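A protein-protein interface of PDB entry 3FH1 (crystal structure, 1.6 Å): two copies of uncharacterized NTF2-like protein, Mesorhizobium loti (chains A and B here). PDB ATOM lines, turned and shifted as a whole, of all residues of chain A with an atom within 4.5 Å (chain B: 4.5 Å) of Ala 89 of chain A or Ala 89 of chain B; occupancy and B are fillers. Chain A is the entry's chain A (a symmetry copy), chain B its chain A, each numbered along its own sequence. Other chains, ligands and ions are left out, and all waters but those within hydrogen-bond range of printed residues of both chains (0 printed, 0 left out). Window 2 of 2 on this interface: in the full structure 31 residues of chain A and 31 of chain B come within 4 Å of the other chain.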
ATOM      1  N   HIS A  11       2.911  -8.072  -3.714  1.00  0.00           N
ATOM      2  CA  HIS A  11       2.233  -8.912  -4.649  1.00  0.00           C
ATOM      3  C   HIS A  11       1.888 -10.197  -3.871  1.00  0.00           C
ATOM      4  O   HIS A  11       2.780 -10.877  -3.377  1.00  0.00           O
ATOM      5  CB  HIS A  11       3.118  -9.192  -5.843  1.00  0.00           C
ATOM      6  CG  HIS A  11       2.491 -10.130  -6.801  1.00  0.00           C
ATOM      7  ND1 HIS A  11       1.399  -9.783  -7.564  1.00  0.00           N
ATOM      8  CD2 HIS A  11       2.738 -11.434  -7.053  1.00  0.00           C
ATOM      9  CE1 HIS A  11       1.011 -10.837  -8.265  1.00  0.00           C
ATOM     10  NE2 HIS A  11       1.813 -11.850  -7.978  1.00  0.00           N
ATOM     11  N   SER A  16       5.446 -13.731   0.450  1.00  0.00           N
ATOM     12  CA  SER A  16       5.569 -12.301   0.273  1.00  0.00           C
ATOM     13  C   SER A  16       5.611 -11.519   1.603  1.00  0.00           C
ATOM     14  O   SER A  16       6.422 -10.580   1.745  1.00  0.00           O
ATOM     15  CB  SER A  16       4.430 -11.759  -0.595  1.00  0.00           C
ATOM     16  OG  SER A  16       4.487 -12.267  -1.926  1.00  0.00           O
ATOM     17  N   PHE A  87       8.828  -3.055  -3.568  1.00  0.00           N
ATOM     18  CA  PHE A  87       7.865  -3.981  -4.199  1.00  0.00           C
ATOM     19  C   PHE A  87       8.318  -5.416  -3.920  1.00  0.00           C
ATOM     20  O   PHE A  87       9.480  -5.760  -4.174  1.00  0.00           O
ATOM     21  CB  PHE A  87       7.747  -3.766  -5.710  1.00  0.00           C
ATOM     22  CG  PHE A  87       6.917  -4.831  -6.381  1.00  0.00           C
ATOM     23  CD1 PHE A  87       5.560  -4.801  -6.239  1.00  0.00           C
ATOM     24  CD2 PHE A  87       7.522  -5.863  -7.102  1.00  0.00           C
ATOM     25  CE1 PHE A  87       4.754  -5.798  -6.796  1.00  0.00           C
ATOM     26  CE2 PHE A  87       6.754  -6.857  -7.687  1.00  0.00           C
ATOM     27  CZ  PHE A  87       5.371  -6.831  -7.536  1.00  0.00           C
ATOM     28  N   VAL A  88       7.426  -6.208  -3.356  1.00  0.00           N
ATOM     29  CA  VAL A  88       7.719  -7.598  -2.954  1.00  0.00           C
ATOM     30  C   VAL A  88       6.865  -8.588  -3.671  1.00  0.00           C
ATOM     31  O   VAL A  88       5.657  -8.363  -3.798  1.00  0.00           O
ATOM     32  CB  VAL A  88       7.470  -7.718  -1.415  1.00  0.00           C
ATOM     33  CG1 VAL A  88       7.563  -9.137  -0.958  1.00  0.00           C
ATOM     34  CG2 VAL A  88       8.452  -6.789  -0.671  1.00  0.00           C
ATOM     35  N   ALA A  89       7.449  -9.709  -4.072  1.00  0.00           N
ATOM     36  CA  ALA A  89       6.700 -10.811  -4.640  1.00  0.00           C
ATOM     37  C   ALA A  89       7.441 -12.103  -4.333  1.00  0.00           C
ATOM     38  O   ALA A  89       8.557 -12.318  -4.795  1.00  0.00           O
ATOM     39  CB  ALA A  89       6.480 -10.621  -6.169  1.00  0.00           C
ATOM     40  N   GLY A  90       6.839 -12.936  -3.497  1.00  0.00           N
ATOM     41  CA  GLY A  90       7.424 -14.211  -3.179  1.00  0.00           C
ATOM     42  C   GLY A  90       8.688 -13.983  -2.402  1.00  0.00           C
ATOM     43  O   GLY A  90       8.672 -13.259  -1.407  1.00  0.00           O
ATOM     44  N   ASP A  91       9.788 -14.584  -2.858  1.00  0.00           N
ATOM     45  CA  ASP A  91      11.099 -14.482  -2.183  1.00  0.00           C
ATOM     46  C   ASP A  91      11.947 -13.345  -2.815  1.00  0.00           C
ATOM     47  O   ASP A  91      13.155 -13.191  -2.533  1.00  0.00           O
ATOM     48  CB  ASP A  91      11.844 -15.807  -2.354  1.00  0.00           C
ATOM     49  CG  ASP A  91      11.287 -16.902  -1.548  1.00  0.00           C
ATOM     50  OD1 ASP A  91      10.852 -16.651  -0.390  1.00  0.00           O
ATOM     51  OD2 ASP A  91      11.327 -18.042  -2.079  1.00  0.00           O
ATOM     52  N   ARG A  92      11.332 -12.479  -3.617  1.00  0.00           N
ATOM     53  CA  ARG A  92      12.053 -11.382  -4.267  1.00  0.00           C
ATOM     54  C   ARG A  92      11.508 -10.019  -3.957  1.00  0.00           C
ATOM     55  O   ARG A  92      10.341  -9.884  -3.600  1.00  0.00           O
ATOM     56  CB  ARG A  92      12.016 -11.588  -5.786  1.00  0.00           C
ATOM     57  CG  ARG A  92      12.755 -12.883  -6.151  1.00  0.00           C
ATOM     58  CD  ARG A  92      13.203 -12.822  -7.517  1.00  0.00           C
ATOM     59  NE  ARG A  92      13.746 -14.078  -7.948  1.00  0.00           N
ATOM     60  CZ  ARG A  92      14.473 -14.163  -9.044  1.00  0.00           C
ATOM     61  NH1 ARG A  92      14.734 -13.074  -9.753  1.00  0.00           N
ATOM     62  NH2 ARG A  92      14.895 -15.344  -9.438  1.00  0.00           N
ATOM     63  N   HIS B  11       6.709 -15.801 -11.112  1.00  0.00           N
ATOM     64  CA  HIS B  11       6.157 -15.926  -9.801  1.00  0.00           C
ATOM     65  C   HIS B  11       4.640 -16.100 -10.010  1.00  0.00           C
ATOM     66  O   HIS B  11       3.992 -15.229 -10.579  1.00  0.00           O
ATOM     67  CB  HIS B  11       6.479 -14.700  -8.976  1.00  0.00           C
ATOM     68  CG  HIS B  11       5.853 -14.745  -7.635  1.00  0.00           C
ATOM     69  ND1 HIS B  11       6.258 -15.630  -6.662  1.00  0.00           N
ATOM     70  CD2 HIS B  11       4.789 -14.081  -7.133  1.00  0.00           C
ATOM     71  CE1 HIS B  11       5.474 -15.494  -5.604  1.00  0.00           C
ATOM     72  NE2 HIS B  11       4.579 -14.554  -5.862  1.00  0.00           N
ATOM     73  N   SER B  16       0.459 -13.055 -14.142  1.00  0.00           N
ATOM     74  CA  SER B  16       1.856 -13.293 -14.429  1.00  0.00           C
ATOM     75  C   SER B  16       2.106 -13.847 -15.848  1.00  0.00           C
ATOM     76  O   SER B  16       3.055 -13.405 -16.528  1.00  0.00           O
ATOM     77  CB  SER B  16       2.469 -14.247 -13.400  1.00  0.00           C
ATOM     78  OG  SER B  16       2.488 -13.679 -12.092  1.00  0.00           O
ATOM     79  N   PHE B  87      12.276 -11.818 -14.766  1.00  0.00           N
ATOM     80  CA  PHE B  87      11.486 -12.264 -13.599  1.00  0.00           C
ATOM     81  C   PHE B  87      10.147 -11.524 -13.608  1.00  0.00           C
ATOM     82  O   PHE B  87      10.121 -10.291 -13.701  1.00  0.00           O
ATOM     83  CB  PHE B  87      12.205 -12.009 -12.273  1.00  0.00           C
ATOM     84  CG  PHE B  87      11.325 -12.284 -11.079  1.00  0.00           C
ATOM     85  CD1 PHE B  87      11.070 -13.579 -10.728  1.00  0.00           C
ATOM     86  CD2 PHE B  87      10.739 -11.238 -10.364  1.00  0.00           C
ATOM     87  CE1 PHE B  87      10.215 -13.883  -9.664  1.00  0.00           C
ATOM     88  CE2 PHE B  87       9.905 -11.500  -9.289  1.00  0.00           C
ATOM     89  CZ  PHE B  87       9.637 -12.820  -8.936  1.00  0.00           C
ATOM     90  N   VAL B  88       9.065 -12.280 -13.569  1.00  0.00           N
ATOM     91  CA  VAL B  88       7.696 -11.734 -13.642  1.00  0.00           C
ATOM     92  C   VAL B  88       6.898 -12.038 -12.420  1.00  0.00           C
ATOM     93  O   VAL B  88       6.943 -13.175 -11.939  1.00  0.00           O
ATOM     94  CB  VAL B  88       6.993 -12.361 -14.890  1.00  0.00           C
ATOM     95  CG1 VAL B  88       5.542 -12.005 -14.933  1.00  0.00           C
ATOM     96  CG2 VAL B  88       7.748 -11.927 -16.165  1.00  0.00           C
ATOM     97  N   ALA B  89       6.112 -11.076 -11.958  1.00  0.00           N
ATOM     98  CA  ALA B  89       5.175 -11.295 -10.875  1.00  0.00           C
ATOM     99  C   ALA B  89       4.006 -10.339 -11.051  1.00  0.00           C
ATOM    100  O   ALA B  89       4.165  -9.125 -10.979  1.00  0.00           O
ATOM    101  CB  ALA B  89       5.859 -11.122  -9.488  1.00  0.00           C
ATOM    102  N   GLY B  90       2.839 -10.892 -11.347  1.00  0.00           N
ATOM    103  CA  GLY B  90       1.655 -10.087 -11.482  1.00  0.00           C
ATOM    104  C   GLY B  90       1.803  -9.209 -12.691  1.00  0.00           C
ATOM    105  O   GLY B  90       2.108  -9.705 -13.774  1.00  0.00           O
ATOM    106  N   ASP B  91       1.603  -7.902 -12.509  1.00  0.00           N
ATOM    107  CA  ASP B  91       1.679  -6.916 -13.608  1.00  0.00           C
ATOM    108  C   ASP B  91       3.094  -6.279 -13.667  1.00  0.00           C
ATOM    109  O   ASP B  91       3.341  -5.293 -14.394  1.00  0.00           O
ATOM    110  CB  ASP B  91       0.652  -5.813 -13.350  1.00  0.00           C
ATOM    111  CG  ASP B  91      -0.738  -6.244 -13.562  1.00  0.00           C
ATOM    112  OD1 ASP B  91      -0.996  -7.038 -14.509  1.00  0.00           O
ATOM    113  OD2 ASP B  91      -1.588  -5.738 -12.784  1.00  0.00           O
ATOM    114  N   ARG B  92       4.071  -6.862 -12.976  1.00  0.00           N
ATOM    115  CA  ARG B  92       5.434  -6.326 -12.962  1.00  0.00           C
ATOM    116  C   ARG B  92       6.481  -7.294 -13.425  1.00  0.00           C
ATOM    117  O   ARG B  92       6.278  -8.504 -13.364  1.00  0.00           O
ATOM    118  CB  ARG B  92       5.782  -5.876 -11.538  1.00  0.00           C
ATOM    119  CG  ARG B  92       4.850  -4.732 -11.114  1.00  0.00           C
ATOM    120  CD  ARG B  92       5.471  -3.955 -10.075  1.00  0.00           C
ATOM    121  NE  ARG B  92       4.565  -2.984  -9.533  1.00  0.00           N
ATOM    122  CZ  ARG B  92       5.004  -1.985  -8.793  1.00  0.00           C
ATOM    123  NH1 ARG B  92       6.302  -1.852  -8.560  1.00  0.00           N
ATOM    124  NH2 ARG B  92       4.133  -1.155  -8.262  1.00  0.00           N
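Of the 8 printed residues of chain B, 5 touch a printed residue of chain A. Hydrophobic or aromatic side chains of chain B that line the printed part of chain A: His 11, Phe 87 and Ala 89. Among the printed residues, no Asp or Glu carboxylate lies within 4 Å of a Lys or Arg side-chain nitrogen of the other chain.
The backbone carbonyl oxygen (O) of His 11 of chain B lies within hydrogen-bond range of the side-chain hydroxyl (OG) of Ser 16 of chain B (2.6 Å). The backbone carbonyl oxygen (O) of Val 88 of chain B lies within hydrogen-bond range of the backbone NH (N) of His 11 of chain B (2.8 Å). N of Gly 90 of chain B sits at hydrogen-bond distance from OG of Ser 16 of chain B. OG of Ser 16 of chain A sits at hydrogen-bond distance from O of His 11 of chain A (2.6 Å). The backbone NH (N) of His 11 of chain A sits at hydrogen-bond distance from the backbone carbonyl oxygen (O) of Val 88 of chain A, 2.8 Å away. OG of Ser 16 of chain A sits at hydrogen-bond distance from N of Gly 90 of chain A (2.9 Å).
Ala 89 of chain A touches just these residues of chain B: His 11 and Ala 89. Ala 89 of chain B touches just these residues of chain A: His 11 and Ala 89. Printed residues of chain A within 4 Å of Phe 87 of chain B: Arg 92. Of the printed residues of chain B, Phe 87 of chain A touches Arg 92 (3.7 Å). Of the printed residues of chain B, Arg 92 of chain A touches Phe 87 (3.7 Å). The nearest residue of chain B that does not touch Ala 89 of chain A is Phe 87 of chain B (4.3 Å).
His 11 of chain B touches its own counterpart, His 11 of chain A. His 11 of chain A touches Ala 89 of chain B, and with the chains exchanged Ala 89 of chain A touches His 11 of chain B. His 11 of chain A touches Gly 90 of chain B, and with the chains exchanged Gly 90 of chain A touches His 11 of chain B. Phe 87 of chain A touches Arg 92 of chain B, and with the chains exchanged Arg 92 of chain A touches Phe 87 of chain B.
Among the printed residues, merely in contact across the chains: His 11 of chain A with His 11 of chain B, His 11 of chain A with Ala 89 of chain B, His 11 of chain A with Gly 90 of chain B, Phe 87 of chain A with Arg 92 of chain B, Ala 89 of chain A with His 11 of chain B, Ala 89 of chain A with Ala 89 of chain B, Gly 90 of chain A with His 11 of chain B and Arg 92 of chain A with Phe 87 of chain B.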
